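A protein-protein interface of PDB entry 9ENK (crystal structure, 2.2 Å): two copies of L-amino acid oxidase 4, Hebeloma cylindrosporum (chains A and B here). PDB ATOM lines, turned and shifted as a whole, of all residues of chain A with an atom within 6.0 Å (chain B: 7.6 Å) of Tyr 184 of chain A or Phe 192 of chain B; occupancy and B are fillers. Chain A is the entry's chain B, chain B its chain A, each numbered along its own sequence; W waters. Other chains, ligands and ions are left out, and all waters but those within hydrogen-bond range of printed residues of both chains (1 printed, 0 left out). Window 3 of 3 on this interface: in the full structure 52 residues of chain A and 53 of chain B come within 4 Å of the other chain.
Asn 181 of chain A touches none of the printed residues of chain B. Of chain B, only Ser 191 (3.8 Å) and Phe 192 (3.7 Å) come within 4 Å of Ala 183 of chain A. Of the printed residues of chain B, Tyr 184 of chain A touches Phe 192 (3.3 Å). Of the printed residues of chain B, Phe 192 of chain A touches Tyr 184. Lys 193 of chain A touches none of the printed residues of chain B. Of the printed residues of chain B, Gly 475 of chain A touches Thr 209 (3.8 Å). Of the printed residues of chain A, Tyr 184 of chain B touches Phe 192 (3.3 Å). Printed residues of chain A within 4 Å of Arg 187 of chain B: Pro 474. Of chain A, only Ala 183 and Tyr 184 come within 4 Å of Phe 192 of chain B. The nearest residue of chain B that does not touch Tyr 184 of chain A is Ser 188 of chain B (6.0 Å).
Printed residues of chain A that touch a printed residue of chain B: Ala 183, Tyr 184, Ser 188, Phe 192, Pro 474 and Gly 475. Hydrophobic or aromatic side chains of chain A that line the printed part of chain B: Ala 183, Tyr 184, Phe 192 and Pro 474. Along chain A the printed residues that touch a printed residue of chain B span positions 183 to 475. Hydrophobic or aromatic side chains of chain B within 4 Å of the printed part of chain A: Tyr 184 and Phe 192. Along chain B the printed residues that touch a printed residue of chain A span positions 184 to 209. Among the printed residues, 7 pairs touch across the chains.
Among the printed residues, pairs that only touch across the chains: Tyr 184 of chain A with Phe 192 of chain B (3.3 Å), Phe 192 of chain A with Tyr 184 of chain B (3.3 Å), Pro 474 of chain A with Arg 187 of chain B (3.5 Å), Ala 183 of chain A with Phe 192 of chain B (3.7 Å), Gly 475 of chain A with Thr 209 of chain B (3.8 Å), Ala 183 of chain A with Ser 191 of chain B (3.8 Å) and Ser 188 of chain A with Ser 188 of chain B (3.9 Å).
Tyr 184 of chain A touches Phe 192 of chain B, and with the chains exchanged Phe 192 of chain A touches Tyr 184 of chain B. Ser 188 of chain A touches its own counterpart, Ser 188 of chain B. 8 positions are printed for both chains. Of the 7 pairs that touch across the chains among the printed residues, 3 have their exchanged pair printed and touching as well.
Water W1 lies within hydrogen-bond range of O of Pro 474 of chain A (2.9 Å) and NE of Arg 187 of chain B (3.3 Å).
The side-chain hydroxyl (OG) of Ser 188 of chain B lies within hydrogen-bond range of the backbone NH (N) of Ser 185 of chain B (2.9 Å). N of Leu 229 of chain A lies within hydrogen-bond range of O of Tyr 184 of chain A (2.9 Å). The backbone NH (N) of Ser 185 of chain A is in hydrogen-bond range of the side-chain hydroxyl (OG) of Ser 188 of chain A (3.0 Å). N of Arg 187 of chain B sits close to OG of Ser 185 of chain B (3.4 Å). A ring nitrogen (NE2) of His 206 of chain B lies within hydrogen-bond range of the backbone carbonyl oxygen (O) of Phe 192 of chain B (3.4 Å). O of Asp 182 of chain A is in hydrogen-bond range of N of Gly 475 of chain A (2.9 Å).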
ATOM      1  N   LYS A 180      20.601 -18.750 -28.631  1.00  0.00           N
ATOM      2  CA  LYS A 180      20.144 -17.584 -29.395  1.00  0.00           C
ATOM      3  C   LYS A 180      19.518 -16.512 -28.515  1.00  0.00           C
ATOM      4  O   LYS A 180      19.528 -15.331 -28.895  1.00  0.00           O
ATOM      5  CB  LYS A 180      19.177 -18.029 -30.501  1.00  0.00           C
ATOM      6  CG  LYS A 180      19.907 -18.680 -31.677  1.00  0.00           C
ATOM      7  CD  LYS A 180      19.042 -18.948 -32.910  1.00  0.00           C
ATOM      8  CE  LYS A 180      20.002 -19.402 -34.051  1.00  0.00           C
ATOM      9  NZ  LYS A 180      19.408 -19.711 -35.390  1.00  0.00           N
ATOM     10  N   ASN A 181      19.038 -16.879 -27.321  1.00  0.00           N
ATOM     11  CA  ASN A 181      18.493 -15.910 -26.383  1.00  0.00           C
ATOM     12  C   ASN A 181      19.413 -15.681 -25.192  1.00  0.00           C
ATOM     13  O   ASN A 181      19.001 -15.048 -24.217  1.00  0.00           O
ATOM     14  CB  ASN A 181      17.130 -16.402 -25.873  1.00  0.00           C
ATOM     15  CG  ASN A 181      16.068 -16.428 -26.959  1.00  0.00           C
ATOM     16  OD1 ASN A 181      15.362 -15.440 -27.178  1.00  0.00           O
ATOM     17  ND2 ASN A 181      15.958 -17.555 -27.651  1.00  0.00           N
ATOM     18  N   ASP A 182      20.661 -16.145 -25.270  1.00  0.00           N
ATOM     19  CA  ASP A 182      21.565 -16.053 -24.129  1.00  0.00           C
ATOM     20  C   ASP A 182      22.035 -14.625 -23.880  1.00  0.00           C
ATOM     21  O   ASP A 182      22.486 -14.317 -22.771  1.00  0.00           O
ATOM     22  CB  ASP A 182      22.779 -16.967 -24.342  1.00  0.00           C
ATOM     23  CG  ASP A 182      23.724 -16.982 -23.149  1.00  0.00           C
ATOM     24  OD1 ASP A 182      23.274 -17.326 -22.031  1.00  0.00           O
ATOM     25  OD2 ASP A 182      24.920 -16.662 -23.335  1.00  0.00           O
ATOM     26  N   ALA A 183      21.927 -13.743 -24.877  1.00  0.00           N
ATOM     27  CA  ALA A 183      22.275 -12.342 -24.669  1.00  0.00           C
ATOM     28  C   ALA A 183      21.271 -11.624 -23.777  1.00  0.00           C
ATOM     29  O   ALA A 183      21.557 -10.517 -23.310  1.00  0.00           O
ATOM     30  CB  ALA A 183      22.383 -11.624 -26.017  1.00  0.00           C
ATOM     31  N   TYR A 184      20.115 -12.231 -23.515  1.00  0.00           N
ATOM     32  CA  TYR A 184      19.153 -11.650 -22.600  1.00  0.00           C
ATOM     33  C   TYR A 184      19.566 -11.901 -21.156  1.00  0.00           C
ATOM     34  O   TYR A 184      20.008 -12.994 -20.800  1.00  0.00           O
ATOM     35  CB  TYR A 184      17.756 -12.244 -22.812  1.00  0.00           C
ATOM     36  CG  TYR A 184      17.021 -11.724 -24.029  1.00  0.00           C
ATOM     37  CD1 TYR A 184      16.499 -10.442 -24.051  1.00  0.00           C
ATOM     38  CD2 TYR A 184      16.850 -12.523 -25.157  1.00  0.00           C
ATOM     39  CE1 TYR A 184      15.825  -9.961 -25.158  1.00  0.00           C
ATOM     40  CE2 TYR A 184      16.170 -12.048 -26.275  1.00  0.00           C
ATOM     41  CZ  TYR A 184      15.670 -10.767 -26.266  1.00  0.00           C
ATOM     42  OH  TYR A 184      15.010 -10.291 -27.364  1.00  0.00           O
ATOM     43  N   SER A 185      19.438 -10.873 -20.328  1.00  0.00           N
ATOM     44  CA  SER A 185      19.221 -11.108 -18.910  1.00  0.00           C
ATOM     45  C   SER A 185      17.746 -11.448 -18.710  1.00  0.00           C
ATOM     46  O   SER A 185      16.914 -11.245 -19.602  1.00  0.00           O
ATOM     47  CB  SER A 185      19.620  -9.897 -18.088  1.00  0.00           C
ATOM     48  OG  SER A 185      18.775  -8.803 -18.365  1.00  0.00           O
ATOM     49  N   THR A 186      17.410 -11.976 -17.536  1.00  0.00           N
ATOM     50  CA  THR A 186      16.002 -12.227 -17.253  1.00  0.00           C
ATOM     51  C   THR A 186      15.200 -10.932 -17.341  1.00  0.00           C
ATOM     52  O   THR A 186      14.089 -10.915 -17.880  1.00  0.00           O
ATOM     53  CB  THR A 186      15.838 -12.878 -15.877  1.00  0.00           C
ATOM     54  OG1 THR A 186      16.597 -14.097 -15.822  1.00  0.00           O
ATOM     55  CG2 THR A 186      14.360 -13.193 -15.605  1.00  0.00           C
ATOM     56  N   SER A 188      15.940  -8.074 -19.120  1.00  0.00           N
ATOM     57  CA  SER A 188      15.795  -7.562 -20.476  1.00  0.00           C
ATOM     58  C   SER A 188      14.891  -8.468 -21.302  1.00  0.00           C
ATOM     59  O   SER A 188      14.200  -7.999 -22.218  1.00  0.00           O
ATOM     60  CB  SER A 188      17.161  -7.412 -21.147  1.00  0.00           C
ATOM     61  OG  SER A 188      17.723  -8.676 -21.421  1.00  0.00           O
ATOM     62  N   TYR A 189      14.861  -9.761 -20.977  1.00  0.00           N
ATOM     63  CA  TYR A 189      13.898 -10.644 -21.624  1.00  0.00           C
ATOM     64  C   TYR A 189      12.470 -10.213 -21.298  1.00  0.00           C
ATOM     65  O   TYR A 189      11.617 -10.113 -22.194  1.00  0.00           O
ATOM     66  CB  TYR A 189      14.129 -12.095 -21.208  1.00  0.00           C
ATOM     67  CG  TYR A 189      13.201 -13.038 -21.929  1.00  0.00           C
ATOM     68  CD1 TYR A 189      13.380 -13.315 -23.286  1.00  0.00           C
ATOM     69  CD2 TYR A 189      12.117 -13.622 -21.273  1.00  0.00           C
ATOM     70  CE1 TYR A 189      12.518 -14.172 -23.970  1.00  0.00           C
ATOM     71  CE2 TYR A 189      11.256 -14.484 -21.945  1.00  0.00           C
ATOM     72  CZ  TYR A 189      11.462 -14.752 -23.287  1.00  0.00           C
ATOM     73  OH  TYR A 189      10.616 -15.594 -23.950  1.00  0.00           O
ATOM     74  N   PHE A 190      12.192  -9.957 -20.016  1.00  0.00           N
ATOM     75  CA  PHE A 190      10.869  -9.479 -19.626  1.00  0.00           C
ATOM     76  C   PHE A 190      10.585  -8.090 -20.196  1.00  0.00           C
ATOM     77  O   PHE A 190       9.437  -7.783 -20.543  1.00  0.00           O
ATOM     78  CB  PHE A 190      10.726  -9.434 -18.098  1.00  0.00           C
ATOM     79  CG  PHE A 190      10.312 -10.736 -17.476  1.00  0.00           C
ATOM     80  CD1 PHE A 190       9.099 -11.318 -17.789  1.00  0.00           C
ATOM     81  CD2 PHE A 190      11.125 -11.363 -16.541  1.00  0.00           C
ATOM     82  CE1 PHE A 190       8.719 -12.510 -17.211  1.00  0.00           C
ATOM     83  CE2 PHE A 190      10.739 -12.551 -15.955  1.00  0.00           C
ATOM     84  CZ  PHE A 190       9.533 -13.122 -16.287  1.00  0.00           C
ATOM     85  N   PHE A 192      11.807  -6.565 -23.006  1.00  0.00           N
ATOM     86  CA  PHE A 192      11.856  -6.357 -24.444  1.00  0.00           C
ATOM     87  C   PHE A 192      11.371  -7.533 -25.280  1.00  0.00           C
ATOM     88  O   PHE A 192      11.269  -7.384 -26.499  1.00  0.00           O
ATOM     89  CB  PHE A 192      13.287  -5.996 -24.871  1.00  0.00           C
ATOM     90  CG  PHE A 192      13.856  -4.839 -24.108  1.00  0.00           C
ATOM     91  CD1 PHE A 192      13.366  -3.557 -24.299  1.00  0.00           C
ATOM     92  CD2 PHE A 192      14.858  -5.036 -23.173  1.00  0.00           C
ATOM     93  CE1 PHE A 192      13.881  -2.488 -23.587  1.00  0.00           C
ATOM     94  CE2 PHE A 192      15.383  -3.967 -22.456  1.00  0.00           C
ATOM     95  CZ  PHE A 192      14.898  -2.700 -22.663  1.00  0.00           C
ATOM     96  N   LYS A 193      11.061  -8.679 -24.682  1.00  0.00           N
ATOM     97  CA  LYS A 193      10.686  -9.839 -25.479  1.00  0.00           C
ATOM     98  C   LYS A 193       9.449 -10.548 -24.945  1.00  0.00           C
ATOM     99  O   LYS A 193       8.481 -10.742 -25.687  1.00  0.00           O
ATOM    100  CB  LYS A 193      11.871 -10.809 -25.547  1.00  0.00           C
ATOM    101  CG  LYS A 193      11.708 -11.972 -26.495  1.00  0.00           C
ATOM    102  CD  LYS A 193      11.603 -11.507 -27.943  1.00  0.00           C
ATOM    103  CE  LYS A 193      11.321 -12.672 -28.884  1.00  0.00           C
ATOM    104  NZ  LYS A 193      12.391 -13.717 -28.793  1.00  0.00           N
ATOM    105  N   ARG A 227      21.343 -11.024 -14.128  1.00  0.00           N
ATOM    106  CA  ARG A 227      22.202 -12.083 -14.625  1.00  0.00           C
ATOM    107  C   ARG A 227      21.547 -12.721 -15.847  1.00  0.00           C
ATOM    108  O   ARG A 227      20.443 -12.344 -16.267  1.00  0.00           O
ATOM    109  CB  ARG A 227      22.465 -13.110 -13.532  1.00  0.00           C
ATOM    110  CG  ARG A 227      22.881 -12.487 -12.223  1.00  0.00           C
ATOM    111  CD  ARG A 227      24.318 -12.724 -11.953  1.00  0.00           C
ATOM    112  NE  ARG A 227      24.798 -11.941 -10.824  1.00  0.00           N
ATOM    113  CZ  ARG A 227      26.026 -12.034 -10.332  1.00  0.00           C
ATOM    114  NH1 ARG A 227      26.897 -12.897 -10.825  1.00  0.00           N
ATOM    115  NH2 ARG A 227      26.384 -11.234  -9.333  1.00  0.00           N
ATOM    116  N   GLY A 228      22.218 -13.723 -16.409  1.00  0.00           N
ATOM    117  CA  GLY A 228      21.758 -14.299 -17.658  1.00  0.00           C
ATOM    118  C   GLY A 228      20.416 -14.993 -17.507  1.00  0.00           C
ATOM    119  O   GLY A 228      20.160 -15.693 -16.525  1.00  0.00           O
ATOM    120  N   LEU A 229      19.557 -14.804 -18.519  1.00  0.00           N
ATOM    121  CA  LEU A 229      18.308 -15.552 -18.598  1.00  0.00           C
ATOM    122  C   LEU A 229      18.571 -17.045 -18.578  1.00  0.00           C
ATOM    123  O   LEU A 229      17.794 -17.816 -18.002  1.00  0.00           O
ATOM    124  CB  LEU A 229      17.553 -15.166 -19.869  1.00  0.00           C
ATOM    125  CG  LEU A 229      16.341 -16.012 -20.273  1.00  0.00           C
ATOM    126  CD1 LEU A 229      15.191 -15.823 -19.276  1.00  0.00           C
ATOM    127  CD2 LEU A 229      15.880 -15.688 -21.703  1.00  0.00           C
ATOM    128  N   THR A 230      19.661 -17.474 -19.202  1.00  0.00           N
ATOM    129  CA  THR A 230      19.953 -18.901 -19.246  1.00  0.00           C
ATOM    130  C   THR A 230      20.120 -19.463 -17.840  1.00  0.00           C
ATOM    131  O   THR A 230      19.685 -20.585 -17.563  1.00  0.00           O
ATOM    132  CB  THR A 230      21.200 -19.161 -20.093  1.00  0.00           C
ATOM    133  OG1 THR A 230      20.963 -18.686 -21.430  1.00  0.00           O
ATOM    134  CG2 THR A 230      21.529 -20.646 -20.123  1.00  0.00           C
ATOM    135  N   GLY A 473      26.601 -14.139 -16.383  1.00  0.00           N
ATOM    136  CA  GLY A 473      25.854 -13.052 -16.950  1.00  0.00           C
ATOM    137  C   GLY A 473      25.417 -13.381 -18.347  1.00  0.00           C
ATOM    138  O   GLY A 473      25.765 -14.426 -18.916  1.00  0.00           O
ATOM    139  N   PRO A 474      24.609 -12.492 -18.926  1.00  0.00           N
ATOM    140  CA  PRO A 474      24.164 -12.707 -20.308  1.00  0.00           C
ATOM    141  C   PRO A 474      25.355 -12.823 -21.247  1.00  0.00           C
ATOM    142  O   PRO A 474      26.315 -12.060 -21.153  1.00  0.00           O
ATOM    143  CB  PRO A 474      23.317 -11.465 -20.616  1.00  0.00           C
ATOM    144  CG  PRO A 474      22.931 -10.911 -19.288  1.00  0.00           C
ATOM    145  CD  PRO A 474      24.036 -11.267 -18.336  1.00  0.00           C
ATOM    146  N   GLY A 475      25.277 -13.786 -22.162  1.00  0.00           N
ATOM    147  CA  GLY A 475      26.300 -13.983 -23.157  1.00  0.00           C
ATOM    148  C   GLY A 475      27.416 -14.928 -22.762  1.00  0.00           C
ATOM    149  O   GLY A 475      28.086 -15.467 -23.644  1.00  0.00           O
ATOM    150  N   TYR B 184      17.384  -0.936 -20.396  1.00  0.00           N
ATOM    151  CA  TYR B 184      18.526  -1.561 -21.036  1.00  0.00           C
ATOM    152  C   TYR B 184      19.736  -1.557 -20.108  1.00  0.00           C
ATOM    153  O   TYR B 184      20.043  -0.548 -19.466  1.00  0.00           O
ATOM    154  CB  TYR B 184      18.909  -0.824 -22.326  1.00  0.00           C
ATOM    155  CG  TYR B 184      18.001  -1.081 -23.506  1.00  0.00           C
ATOM    156  CD1 TYR B 184      18.029  -2.296 -24.174  1.00  0.00           C
ATOM    157  CD2 TYR B 184      17.116  -0.107 -23.948  1.00  0.00           C
ATOM    158  CE1 TYR B 184      17.201  -2.542 -25.239  1.00  0.00           C
ATOM    159  CE2 TYR B 184      16.283  -0.344 -25.025  1.00  0.00           C
ATOM    160  CZ  TYR B 184      16.332  -1.564 -25.663  1.00  0.00           C
ATOM    161  OH  TYR B 184      15.515  -1.809 -26.737  1.00  0.00           O
ATOM    162  N   SER B 185      20.438  -2.686 -20.060  1.00  0.00           N
ATOM    163  CA  SER B 185      21.841  -2.626 -19.695  1.00  0.00           C
ATOM    164  C   SER B 185      22.622  -2.160 -20.920  1.00  0.00           C
ATOM    165  O   SER B 185      22.103  -2.131 -22.038  1.00  0.00           O
ATOM    166  CB  SER B 185      22.349  -3.979 -19.213  1.00  0.00           C
ATOM    167  OG  SER B 185      22.333  -4.934 -20.265  1.00  0.00           O
ATOM    168  N   THR B 186      23.879  -1.773 -20.711  1.00  0.00           N
ATOM    169  CA  THR B 186      24.708  -1.434 -21.861  1.00  0.00           C
ATOM    170  C   THR B 186      24.801  -2.621 -22.806  1.00  0.00           C
ATOM    171  O   THR B 186      24.736  -2.456 -24.028  1.00  0.00           O
ATOM    172  CB  THR B 186      26.084  -0.981 -21.406  1.00  0.00           C
ATOM    173  OG1 THR B 186      25.931   0.110 -20.494  1.00  0.00           O
ATOM    174  CG2 THR B 186      26.924  -0.497 -22.592  1.00  0.00           C
ATOM    175  N   ARG B 187      24.909  -3.830 -22.250  1.00  0.00           N
ATOM    176  CA  ARG B 187      25.019  -5.031 -23.069  1.00  0.00           C
ATOM    177  C   ARG B 187      23.739  -5.287 -23.856  1.00  0.00           C
ATOM    178  O   ARG B 187      23.783  -5.514 -25.072  1.00  0.00           O
ATOM    179  CB  ARG B 187      25.366  -6.237 -22.183  1.00  0.00           C
ATOM    180  CG  ARG B 187      25.290  -7.593 -22.893  1.00  0.00           C
ATOM    181  CD  ARG B 187      25.603  -8.741 -21.930  1.00  0.00           C
ATOM    182  NE  ARG B 187      26.933  -8.590 -21.344  1.00  0.00           N
ATOM    183  CZ  ARG B 187      28.057  -8.889 -21.979  1.00  0.00           C
ATOM    184  NH1 ARG B 187      28.045  -9.367 -23.215  1.00  0.00           N
ATOM    185  NH2 ARG B 187      29.222  -8.701 -21.359  1.00  0.00           N
ATOM    186  N   SER B 188      22.589  -5.266 -23.183  1.00  0.00           N
ATOM    187  CA  SER B 188      21.348  -5.555 -23.879  1.00  0.00           C
ATOM    188  C   SER B 188      21.027  -4.460 -24.889  1.00  0.00           C
ATOM    189  O   SER B 188      20.400  -4.734 -25.918  1.00  0.00           O
ATOM    190  CB  SER B 188      20.200  -5.733 -22.877  1.00  0.00           C
ATOM    191  OG  SER B 188      19.867  -4.508 -22.251  1.00  0.00           O
ATOM    192  N   TYR B 189      21.470  -3.225 -24.630  1.00  0.00           N
ATOM    193  CA  TYR B 189      21.334  -2.173 -25.633  1.00  0.00           C
ATOM    194  C   TYR B 189      22.134  -2.507 -26.893  1.00  0.00           C
ATOM    195  O   TYR B 189      21.627  -2.384 -28.016  1.00  0.00           O
ATOM    196  CB  TYR B 189      21.781  -0.823 -25.060  1.00  0.00           C
ATOM    197  CG  TYR B 189      21.582   0.315 -26.037  1.00  0.00           C
ATOM    198  CD1 TYR B 189      20.304   0.781 -26.340  1.00  0.00           C
ATOM    199  CD2 TYR B 189      22.662   0.918 -26.660  1.00  0.00           C
ATOM    200  CE1 TYR B 189      20.116   1.812 -27.247  1.00  0.00           C
ATOM    201  CE2 TYR B 189      22.485   1.950 -27.559  1.00  0.00           C
ATOM    202  CZ  TYR B 189      21.210   2.386 -27.854  1.00  0.00           C
ATOM    203  OH  TYR B 189      21.023   3.405 -28.746  1.00  0.00           O
ATOM    204  N   PHE B 190      23.392  -2.917 -26.728  1.00  0.00           N
ATOM    205  CA  PHE B 190      24.197  -3.305 -27.884  1.00  0.00           C
ATOM    206  C   PHE B 190      23.640  -4.553 -28.561  1.00  0.00           C
ATOM    207  O   PHE B 190      23.694  -4.676 -29.789  1.00  0.00           O
ATOM    208  CB  PHE B 190      25.656  -3.565 -27.477  1.00  0.00           C
ATOM    209  CG  PHE B 190      26.516  -2.337 -27.444  1.00  0.00           C
ATOM    210  CD1 PHE B 190      26.717  -1.584 -28.595  1.00  0.00           C
ATOM    211  CD2 PHE B 190      27.160  -1.958 -26.283  1.00  0.00           C
ATOM    212  CE1 PHE B 190      27.508  -0.457 -28.569  1.00  0.00           C
ATOM    213  CE2 PHE B 190      27.968  -0.835 -26.255  1.00  0.00           C
ATOM    214  CZ  PHE B 190      28.152  -0.089 -27.393  1.00  0.00           C
ATOM    215  N   SER B 191      23.101  -5.492 -27.782  1.00  0.00           N
ATOM    216  CA  SER B 191      22.688  -6.777 -28.345  1.00  0.00           C
ATOM    217  C   SER B 191      21.349  -6.691 -29.068  1.00  0.00           C
ATOM    218  O   SER B 191      21.112  -7.456 -30.010  1.00  0.00           O
ATOM    219  CB  SER B 191      22.587  -7.841 -27.249  1.00  0.00           C
ATOM    220  OG  SER B 191      23.852  -8.181 -26.740  1.00  0.00           O
ATOM    221  N   PHE B 192      20.469  -5.773 -28.647  1.00  0.00           N
ATOM    222  CA  PHE B 192      19.104  -5.748 -29.141  1.00  0.00           C
ATOM    223  C   PHE B 192      18.630  -4.422 -29.712  1.00  0.00           C
ATOM    224  O   PHE B 192      17.515  -4.379 -30.238  1.00  0.00           O
ATOM    225  CB  PHE B 192      18.132  -6.182 -28.026  1.00  0.00           C
ATOM    226  CG  PHE B 192      18.433  -7.530 -27.469  1.00  0.00           C
ATOM    227  CD1 PHE B 192      18.221  -8.669 -28.241  1.00  0.00           C
ATOM    228  CD2 PHE B 192      18.945  -7.672 -26.196  1.00  0.00           C
ATOM    229  CE1 PHE B 192      18.512  -9.929 -27.737  1.00  0.00           C
ATOM    230  CE2 PHE B 192      19.236  -8.920 -25.689  1.00  0.00           C
ATOM    231  CZ  PHE B 192      19.016 -10.055 -26.458  1.00  0.00           C
ATOM    232  N   LYS B 193      19.404  -3.345 -29.614  1.00  0.00           N
ATOM    233  CA  LYS B 193      18.910  -2.083 -30.148  1.00  0.00           C
ATOM    234  C   LYS B 193      19.934  -1.337 -30.988  1.00  0.00           C
ATOM    235  O   LYS B 193      19.623  -0.922 -32.108  1.00  0.00           O
ATOM    236  CB  LYS B 193      18.391  -1.187 -29.018  1.00  0.00           C
ATOM    237  CG  LYS B 193      17.679   0.052 -29.548  1.00  0.00           C
ATOM    238  CD  LYS B 193      16.931   0.794 -28.459  1.00  0.00           C
ATOM    239  CE  LYS B 193      16.225   2.013 -29.039  1.00  0.00           C
ATOM    240  NZ  LYS B 193      15.477   2.778 -28.002  1.00  0.00           N
ATOM    241  N   TYR B 194      21.135  -1.143 -30.455  1.00  0.00           N
ATOM    242  CA  TYR B 194      22.135  -0.335 -31.144  1.00  0.00           C
ATOM    243  C   TYR B 194      22.438  -0.882 -32.531  1.00  0.00           C
ATOM    244  O   TYR B 194      22.607  -2.091 -32.723  1.00  0.00           O
ATOM    245  CB  TYR B 194      23.432  -0.263 -30.334  1.00  0.00           C
ATOM    246  CG  TYR B 194      24.552   0.453 -31.064  1.00  0.00           C
ATOM    247  CD1 TYR B 194      24.567   1.839 -31.164  1.00  0.00           C
ATOM    248  CD2 TYR B 194      25.584  -0.257 -31.666  1.00  0.00           C
ATOM    249  CE1 TYR B 194      25.590   2.498 -31.831  1.00  0.00           C
ATOM    250  CE2 TYR B 194      26.601   0.387 -32.340  1.00  0.00           C
ATOM    251  CZ  TYR B 194      26.607   1.763 -32.412  1.00  0.00           C
ATOM    252  OH  TYR B 194      27.622   2.410 -33.086  1.00  0.00           O
ATOM    253  N   LEU B 195      22.510   0.023 -33.503  1.00  0.00           N
ATOM    254  CA  LEU B 195      22.963  -0.290 -34.849  1.00  0.00           C
ATOM    255  C   LEU B 195      24.066   0.698 -35.210  1.00  0.00           C
ATOM    256  O   LEU B 195      23.929   1.905 -34.940  1.00  0.00           O
ATOM    257  CB  LEU B 195      21.817  -0.222 -35.867  1.00  0.00           C
ATOM    258  CG  LEU B 195      20.772  -1.327 -35.706  1.00  0.00           C
ATOM    259  CD1 LEU B 195      19.579  -1.105 -36.624  1.00  0.00           C
ATOM    260  CD2 LEU B 195      21.395  -2.701 -35.968  1.00  0.00           C
ATOM    261  N   HIS B 206      23.048  -5.896 -35.053  1.00  0.00           N
ATOM    262  CA  HIS B 206      23.517  -5.706 -33.691  1.00  0.00           C
ATOM    263  C   HIS B 206      24.817  -6.475 -33.481  1.00  0.00           C
ATOM    264  O   HIS B 206      24.993  -7.584 -33.990  1.00  0.00           O
ATOM    265  CB  HIS B 206      22.463  -6.175 -32.689  1.00  0.00           C
ATOM    266  CG  HIS B 206      21.123  -5.556 -32.895  1.00  0.00           C
ATOM    267  ND1 HIS B 206      20.930  -4.193 -32.894  1.00  0.00           N
ATOM    268  CD2 HIS B 206      19.907  -6.111 -33.104  1.00  0.00           C
ATOM    269  CE1 HIS B 206      19.652  -3.935 -33.097  1.00  0.00           C
ATOM    270  NE2 HIS B 206      19.011  -5.081 -33.230  1.00  0.00           N
ATOM    271  N   PHE B 207      25.710  -5.897 -32.692  1.00  0.00           N
ATOM    272  CA  PHE B 207      26.983  -6.541 -32.416  1.00  0.00           C
ATOM    273  C   PHE B 207      26.764  -7.891 -31.745  1.00  0.00           C
ATOM    274  O   PHE B 207      25.822  -8.086 -30.960  1.00  0.00           O
ATOM    275  CB  PHE B 207      27.836  -5.657 -31.503  1.00  0.00           C
ATOM    276  CG  PHE B 207      28.361  -4.419 -32.156  1.00  0.00           C
ATOM    277  CD1 PHE B 207      28.650  -4.389 -33.511  1.00  0.00           C
ATOM    278  CD2 PHE B 207      28.562  -3.269 -31.408  1.00  0.00           C
ATOM    279  CE1 PHE B 207      29.135  -3.237 -34.106  1.00  0.00           C
ATOM    280  CE2 PHE B 207      29.035  -2.120 -31.998  1.00  0.00           C
ATOM    281  CZ  PHE B 207      29.322  -2.105 -33.355  1.00  0.00           C
ATOM    282  N   THR B 209      27.913 -10.966 -29.102  1.00  0.00           N
ATOM    283  CA  THR B 209      28.421 -10.956 -27.736  1.00  0.00           C
ATOM    284  C   THR B 209      29.941 -10.895 -27.717  1.00  0.00           C
ATOM    285  O   THR B 209      30.533 -10.201 -26.879  1.00  0.00           O
ATOM    286  CB  THR B 209      27.927 -12.178 -26.971  1.00  0.00           C
ATOM    287  OG1 THR B 209      26.505 -12.079 -26.776  1.00  0.00           O
ATOM    288  CG2 THR B 209      28.618 -12.272 -25.621  1.00  0.00           C
ATOM    289  N   ILE B 212      30.777  -7.359 -28.226  1.00  0.00           N
ATOM    290  CA  ILE B 212      30.384  -6.542 -27.084  1.00  0.00           C
ATOM    291  C   ILE B 212      31.354  -6.756 -25.930  1.00  0.00           C
ATOM    292  O   ILE B 212      31.747  -5.803 -25.247  1.00  0.00           O
ATOM    293  CB  ILE B 212      28.926  -6.837 -26.675  1.00  0.00           C
ATOM    294  CG1 ILE B 212      27.969  -6.314 -27.749  1.00  0.00           C
ATOM    295  CG2 ILE B 212      28.596  -6.202 -25.354  1.00  0.00           C
ATOM    296  CD1 ILE B 212      26.539  -6.799 -27.618  1.00  0.00           C
HETATM  297  O   HOH W   1      27.596 -10.712 -18.962  1.00  0.00           O
